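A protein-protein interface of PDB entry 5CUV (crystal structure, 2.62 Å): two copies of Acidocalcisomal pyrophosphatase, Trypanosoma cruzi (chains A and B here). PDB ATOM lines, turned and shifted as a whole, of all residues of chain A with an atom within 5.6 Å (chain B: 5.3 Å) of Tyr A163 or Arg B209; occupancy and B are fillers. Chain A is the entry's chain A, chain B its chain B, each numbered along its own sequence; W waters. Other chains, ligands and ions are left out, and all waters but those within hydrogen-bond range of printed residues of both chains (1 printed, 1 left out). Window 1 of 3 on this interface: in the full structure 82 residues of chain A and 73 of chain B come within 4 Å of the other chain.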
ATOM      1  N   VAL A 161      -5.579 -20.419  12.537  1.00  0.00           N
ATOM      2  CA  VAL A 161      -4.578 -21.190  11.854  1.00  0.00           C
ATOM      3  C   VAL A 161      -4.498 -20.813  10.399  1.00  0.00           C
ATOM      4  O   VAL A 161      -5.165 -21.409   9.556  1.00  0.00           O
ATOM      5  CB  VAL A 161      -4.907 -22.651  12.003  1.00  0.00           C
ATOM      6  CG1 VAL A 161      -4.838 -23.021  13.502  1.00  0.00           C
ATOM      7  CG2 VAL A 161      -6.304 -22.912  11.456  1.00  0.00           C
ATOM      8  N   PRO A 162      -3.667 -19.799  10.088  1.00  0.00           N
ATOM      9  CA  PRO A 162      -3.387 -19.218   8.764  1.00  0.00           C
ATOM     10  C   PRO A 162      -2.365 -20.021   7.922  1.00  0.00           C
ATOM     11  O   PRO A 162      -1.602 -20.835   8.446  1.00  0.00           O
ATOM     12  CB  PRO A 162      -2.850 -17.847   9.130  1.00  0.00           C
ATOM     13  CG  PRO A 162      -2.022 -18.183  10.327  1.00  0.00           C
ATOM     14  CD  PRO A 162      -2.973 -19.019  11.131  1.00  0.00           C
ATOM     15  N   TYR A 163      -2.339 -19.790   6.620  1.00  0.00           N
ATOM     16  CA  TYR A 163      -1.373 -20.514   5.801  1.00  0.00           C
ATOM     17  C   TYR A 163      -1.436 -20.199   4.327  1.00  0.00           C
ATOM     18  O   TYR A 163      -2.520 -20.013   3.746  1.00  0.00           O
ATOM     19  CB  TYR A 163      -1.533 -22.030   5.973  1.00  0.00           C
ATOM     20  CG  TYR A 163      -2.839 -22.597   5.453  1.00  0.00           C
ATOM     21  CD1 TYR A 163      -2.991 -22.952   4.105  1.00  0.00           C
ATOM     22  CD2 TYR A 163      -3.916 -22.820   6.327  1.00  0.00           C
ATOM     23  CE1 TYR A 163      -4.184 -23.525   3.635  1.00  0.00           C
ATOM     24  CE2 TYR A 163      -5.112 -23.391   5.877  1.00  0.00           C
ATOM     25  CZ  TYR A 163      -5.242 -23.747   4.534  1.00  0.00           C
ATOM     26  OH  TYR A 163      -6.407 -24.361   4.120  1.00  0.00           O
ATOM     27  N   HIS A 164      -0.265 -20.156   3.714  1.00  0.00           N
ATOM     28  CA  HIS A 164      -0.238 -19.891   2.301  1.00  0.00           C
ATOM     29  C   HIS A 164      -0.584 -21.207   1.641  1.00  0.00           C
ATOM     30  O   HIS A 164       0.066 -22.237   1.895  1.00  0.00           O
ATOM     31  CB  HIS A 164       1.148 -19.391   1.898  1.00  0.00           C
ATOM     32  CG  HIS A 164       1.424 -17.986   2.342  1.00  0.00           C
ATOM     33  ND1 HIS A 164       1.004 -17.497   3.565  1.00  0.00           N
ATOM     34  CD2 HIS A 164       2.053 -16.959   1.722  1.00  0.00           C
ATOM     35  CE1 HIS A 164       1.359 -16.229   3.674  1.00  0.00           C
ATOM     36  NE2 HIS A 164       1.996 -15.878   2.570  1.00  0.00           N
ATOM     37  N   GLN A 165      -1.648 -21.187   0.846  1.00  0.00           N
ATOM     38  CA  GLN A 165      -2.087 -22.370   0.115  1.00  0.00           C
ATOM     39  C   GLN A 165      -1.186 -22.492  -1.094  1.00  0.00           C
ATOM     40  O   GLN A 165      -0.693 -21.493  -1.594  1.00  0.00           O
ATOM     41  CB  GLN A 165      -3.520 -22.182  -0.319  1.00  0.00           C
ATOM     42  CG  GLN A 165      -4.043 -23.140  -1.382  1.00  0.00           C
ATOM     43  CD  GLN A 165      -5.545 -22.991  -1.506  1.00  0.00           C
ATOM     44  OE1 GLN A 165      -6.075 -21.894  -1.311  1.00  0.00           O
ATOM     45  NE2 GLN A 165      -6.242 -24.076  -1.825  1.00  0.00           N
ATOM     46  N   GLU A 191      -0.405 -16.788  -2.583  1.00  0.00           N
ATOM     47  CA  GLU A 191      -0.465 -15.565  -1.818  1.00  0.00           C
ATOM     48  C   GLU A 191       0.565 -14.660  -2.481  1.00  0.00           C
ATOM     49  O   GLU A 191       0.223 -13.635  -3.079  1.00  0.00           O
ATOM     50  CB  GLU A 191      -0.177 -15.677  -0.330  1.00  0.00           C
ATOM     51  CG  GLU A 191      -0.951 -14.656   0.450  1.00  0.00           C
ATOM     52  CD  GLU A 191      -1.215 -15.122   1.862  1.00  0.00           C
ATOM     53  OE1 GLU A 191      -0.608 -14.512   2.792  1.00  0.00           O
ATOM     54  OE2 GLU A 191      -2.016 -16.096   2.028  1.00  0.00           O
ATOM     55  N   ARG A 209      -6.154 -33.731   3.056  1.00  0.00           N
ATOM     56  CA  ARG A 209      -6.820 -33.351   4.266  1.00  0.00           C
ATOM     57  C   ARG A 209      -7.459 -32.007   4.453  1.00  0.00           C
ATOM     58  O   ARG A 209      -6.820 -31.007   4.325  1.00  0.00           O
ATOM     59  CB  ARG A 209      -5.862 -33.567   5.430  1.00  0.00           C
ATOM     60  CG  ARG A 209      -5.942 -34.938   6.045  1.00  0.00           C
ATOM     61  CD  ARG A 209      -5.086 -34.961   7.298  1.00  0.00           C
ATOM     62  NE  ARG A 209      -4.237 -36.152   7.357  1.00  0.00           N
ATOM     63  CZ  ARG A 209      -2.945 -36.129   7.675  1.00  0.00           C
ATOM     64  NH1 ARG A 209      -2.360 -34.959   7.966  1.00  0.00           N
ATOM     65  NH2 ARG A 209      -2.245 -37.272   7.682  1.00  0.00           N
ATOM     66  N   ASP A 210      -8.727 -32.010   4.824  1.00  0.00           N
ATOM     67  CA  ASP A 210      -9.430 -30.773   5.105  1.00  0.00           C
ATOM     68  C   ASP A 210      -9.133 -30.285   6.515  1.00  0.00           C
ATOM     69  O   ASP A 210      -9.281 -31.039   7.471  1.00  0.00           O
ATOM     70  CB  ASP A 210     -10.924 -30.975   4.962  1.00  0.00           C
ATOM     71  CG  ASP A 210     -11.325 -31.195   3.520  1.00  0.00           C
ATOM     72  OD1 ASP A 210     -10.858 -30.353   2.691  1.00  0.00           O
ATOM     73  OD2 ASP A 210     -12.078 -32.183   3.215  1.00  0.00           O
ATOM     74  N   LEU A 211      -8.714 -29.026   6.613  1.00  0.00           N
ATOM     75  CA  LEU A 211      -8.406 -28.371   7.853  1.00  0.00           C
ATOM     76  C   LEU A 211      -9.569 -28.499   8.793  1.00  0.00           C
ATOM     77  O   LEU A 211      -9.385 -28.752  10.001  1.00  0.00           O
ATOM     78  CB  LEU A 211      -8.131 -26.914   7.588  1.00  0.00           C
ATOM     79  CG  LEU A 211      -7.424 -26.137   8.715  1.00  0.00           C
ATOM     80  CD1 LEU A 211      -6.044 -26.740   9.052  1.00  0.00           C
ATOM     81  CD2 LEU A 211      -7.296 -24.664   8.246  1.00  0.00           C
ATOM     82  N   PHE B 159       7.356 -27.751   3.505  1.00  0.00           N
ATOM     83  CA  PHE B 159       6.105 -27.104   3.774  1.00  0.00           C
ATOM     84  C   PHE B 159       5.073 -27.992   4.451  1.00  0.00           C
ATOM     85  O   PHE B 159       4.062 -28.356   3.845  1.00  0.00           O
ATOM     86  CB  PHE B 159       5.491 -26.538   2.488  1.00  0.00           C
ATOM     87  CG  PHE B 159       4.282 -25.665   2.737  1.00  0.00           C
ATOM     88  CD1 PHE B 159       4.089 -25.055   3.994  1.00  0.00           C
ATOM     89  CD2 PHE B 159       3.332 -25.447   1.733  1.00  0.00           C
ATOM     90  CE1 PHE B 159       2.974 -24.248   4.242  1.00  0.00           C
ATOM     91  CE2 PHE B 159       2.203 -24.634   1.977  1.00  0.00           C
ATOM     92  CZ  PHE B 159       2.028 -24.037   3.230  1.00  0.00           C
ATOM     93  N   VAL B 161       2.495 -28.408   7.798  1.00  0.00           N
ATOM     94  CA  VAL B 161       1.797 -27.437   8.589  1.00  0.00           C
ATOM     95  C   VAL B 161       1.476 -28.156   9.902  1.00  0.00           C
ATOM     96  O   VAL B 161       0.881 -29.218   9.917  1.00  0.00           O
ATOM     97  CB  VAL B 161       0.557 -26.912   7.841  1.00  0.00           C
ATOM     98  CG1 VAL B 161       0.975 -25.806   6.896  1.00  0.00           C
ATOM     99  CG2 VAL B 161      -0.080 -28.022   7.050  1.00  0.00           C
ATOM    100  N   TYR B 163      -0.762 -27.739  12.052  1.00  0.00           N
ATOM    101  CA  TYR B 163      -2.175 -27.791  12.484  1.00  0.00           C
ATOM    102  C   TYR B 163      -2.876 -29.150  12.420  1.00  0.00           C
ATOM    103  O   TYR B 163      -2.760 -29.850  11.424  1.00  0.00           O
ATOM    104  CB  TYR B 163      -3.025 -26.784  11.688  1.00  0.00           C
ATOM    105  CG  TYR B 163      -2.427 -25.397  11.484  1.00  0.00           C
ATOM    106  CD1 TYR B 163      -1.837 -24.705  12.546  1.00  0.00           C
ATOM    107  CD2 TYR B 163      -2.461 -24.767  10.227  1.00  0.00           C
ATOM    108  CE1 TYR B 163      -1.289 -23.427  12.375  1.00  0.00           C
ATOM    109  CE2 TYR B 163      -1.917 -23.475  10.047  1.00  0.00           C
ATOM    110  CZ  TYR B 163      -1.332 -22.822  11.144  1.00  0.00           C
ATOM    111  OH  TYR B 163      -0.797 -21.568  11.033  1.00  0.00           O
ATOM    112  N   TYR B 207     -13.935 -20.192   3.080  1.00  0.00           N
ATOM    113  CA  TYR B 207     -13.329 -20.766   1.883  1.00  0.00           C
ATOM    114  C   TYR B 207     -12.842 -22.160   2.251  1.00  0.00           C
ATOM    115  O   TYR B 207     -12.312 -22.374   3.362  1.00  0.00           O
ATOM    116  CB  TYR B 207     -12.154 -19.918   1.423  1.00  0.00           C
ATOM    117  CG  TYR B 207     -12.538 -18.505   1.038  1.00  0.00           C
ATOM    118  CD1 TYR B 207     -13.014 -18.209  -0.254  1.00  0.00           C
ATOM    119  CD2 TYR B 207     -12.441 -17.445   1.966  1.00  0.00           C
ATOM    120  CE1 TYR B 207     -13.377 -16.902  -0.617  1.00  0.00           C
ATOM    121  CE2 TYR B 207     -12.810 -16.117   1.604  1.00  0.00           C
ATOM    122  CZ  TYR B 207     -13.270 -15.873   0.309  1.00  0.00           C
ATOM    123  OH  TYR B 207     -13.569 -14.587  -0.079  1.00  0.00           O
ATOM    124  N   VAL B 208     -13.068 -23.128   1.368  1.00  0.00           N
ATOM    125  CA  VAL B 208     -12.631 -24.474   1.659  1.00  0.00           C
ATOM    126  C   VAL B 208     -11.341 -24.546   0.869  1.00  0.00           C
ATOM    127  O   VAL B 208     -11.323 -24.612  -0.354  1.00  0.00           O
ATOM    128  CB  VAL B 208     -13.722 -25.495   1.262  1.00  0.00           C
ATOM    129  CG1 VAL B 208     -13.267 -26.953   1.548  1.00  0.00           C
ATOM    130  CG2 VAL B 208     -15.001 -25.175   2.070  1.00  0.00           C
ATOM    131  N   ARG B 209     -10.251 -24.451   1.602  1.00  0.00           N
ATOM    132  CA  ARG B 209      -8.954 -24.412   0.998  1.00  0.00           C
ATOM    133  C   ARG B 209      -8.116 -25.673   1.140  1.00  0.00           C
ATOM    134  O   ARG B 209      -8.022 -26.282   2.216  1.00  0.00           O
ATOM    135  CB  ARG B 209      -8.194 -23.218   1.571  1.00  0.00           C
ATOM    136  CG  ARG B 209      -8.890 -21.873   1.393  1.00  0.00           C
ATOM    137  CD  ARG B 209      -7.926 -20.743   0.971  1.00  0.00           C
ATOM    138  NE  ARG B 209      -8.423 -19.925  -0.164  1.00  0.00           N
ATOM    139  CZ  ARG B 209      -8.891 -18.669  -0.066  1.00  0.00           C
ATOM    140  NH1 ARG B 209      -8.944 -18.039   1.125  1.00  0.00           N
ATOM    141  NH2 ARG B 209      -9.313 -18.031  -1.166  1.00  0.00           N
ATOM    142  N   ASP B 210      -7.531 -26.107   0.039  1.00  0.00           N
ATOM    143  CA  ASP B 210      -6.647 -27.266   0.129  1.00  0.00           C
ATOM    144  C   ASP B 210      -5.253 -26.733   0.490  1.00  0.00           C
ATOM    145  O   ASP B 210      -4.853 -25.651   0.030  1.00  0.00           O
ATOM    146  CB  ASP B 210      -6.521 -28.024  -1.205  1.00  0.00           C
ATOM    147  CG  ASP B 210      -7.817 -28.652  -1.658  1.00  0.00           C
ATOM    148  OD1 ASP B 210      -8.329 -29.574  -0.947  1.00  0.00           O
ATOM    149  OD2 ASP B 210      -8.303 -28.214  -2.746  1.00  0.00           O
ATOM    150  N   LEU B 211      -4.542 -27.481   1.325  1.00  0.00           N
ATOM    151  CA  LEU B 211      -3.194 -27.114   1.688  1.00  0.00           C
ATOM    152  C   LEU B 211      -2.435 -27.169   0.375  1.00  0.00           C
ATOM    153  O   LEU B 211      -1.608 -26.317   0.113  1.00  0.00           O
ATOM    154  CB  LEU B 211      -2.627 -28.122   2.691  1.00  0.00           C
ATOM    155  CG  LEU B 211      -3.759 -28.563   3.661  1.00  0.00           C
ATOM    156  CD1 LEU B 211      -3.313 -29.783   4.451  1.00  0.00           C
ATOM    157  CD2 LEU B 211      -4.161 -27.425   4.634  1.00  0.00           C
ATOM    158  N   MET B 221     -10.845 -21.076  -8.186  1.00  0.00           N
ATOM    159  CA  MET B 221     -11.264 -21.610  -6.988  1.00  0.00           C
ATOM    160  C   MET B 221     -12.576 -21.279  -6.697  1.00  0.00           C
ATOM    161  O   MET B 221     -12.863 -20.268  -6.766  1.00  0.00           O
ATOM    162  CB  MET B 221     -10.398 -21.039  -5.980  1.00  0.00           C
ATOM    163  CG  MET B 221      -9.924 -21.953  -4.919  1.00  0.00           C
ATOM    164  SD  MET B 221      -8.462 -21.395  -3.793  1.00  0.00           S
ATOM    165  CE  MET B 221      -9.312 -22.023  -2.311  1.00  0.00           C
HETATM  166  O   HOH W   1      -6.367 -30.258   1.568  1.00  0.00           O
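The side-chain hydroxyl of Tyr B163 lies within hydrogen-bond range of the backbone carbonyl oxygen of Pro A162 (2.8 Å). O of Arg B209 sits at hydrogen-bond distance from OH of Tyr A163 (3.2 Å). O of Asp B210 is in hydrogen-bond range of NE2 of Gln A165 (2.8 Å). The side-chain amide oxygen of Gln A165 lies close to the side-chain sulfur of Met B221 (3.5 Å). The guanidinium group (NE) of Arg B209 sits close to the side-chain amide oxygen (OE1) of Gln A165.
A ring nitrogen (NE2) of His A164 sits close to the side-chain carboxylate of Glu A191 (2.9 Å).
Among the printed residues, pairs that only touch across the chains: Val A161 with Tyr B163, Tyr A163 with Leu B211, His A164 with Phe B159, Gln A165 with Leu B211 and Arg A209 with Leu B211.
Tyr A163 touches two residues of chain B. Arg B209 touches two residues of chain A. Of the printed residues of chain A, Asp B210 touches Gln A165 (2.8 Å). Of the printed residues of chain A, Phe B159 touches His A164 (3.0 Å). Printed residues of chain B within 4 Å of Val A161: Tyr B163 (3.6 Å). Val B208 touches none of the printed residues of chain A. Asp A210 touches none of the printed residues of chain B. The nearest residue of chain B that does not touch Tyr A163 is Asp B210 (4.2 Å). The nearest residue of chain A that does not touch Arg B209 is Asp A210 (5.0 Å). The nearest printed residue of chain B that does not touch Gln A165 is Phe B159 (5.1 Å).
Hydrophobic or aromatic side chains of chain A that line the printed part of chain B: Val A161, Pro A162 and Tyr A163. Among the printed residues, no Asp or Glu carboxylate lies within 4 Å of a Lys or Arg side-chain nitrogen of the other chain.
Val A161 touches Tyr B163, but with the chains exchanged Tyr A163 does not touch Val B161 (4.6 Å). Tyr A163 touches Arg B209, but with the chains exchanged Arg A209 does not touch Tyr B163 (6.2 Å). Tyr A163 touches Leu B211, but with the chains exchanged Leu A211 does not touch Tyr B163 (4.01 Å). Arg A209 touches Leu B211, but with the chains exchanged Leu A211 does not touch Arg B209 (5.2 Å). 5 positions are printed for both chains. Of the 10 pairs that touch across the chains among the printed residues, none has its exchanged pair printed and touching as well.
Water W1 lies within hydrogen-bond range of the backbone carbonyl oxygen of Arg A209 (2.9 Å), the side-chain carboxylate of Asp B210 (3.3 Å) and the backbone NH of Leu B211 (3.3 Å).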
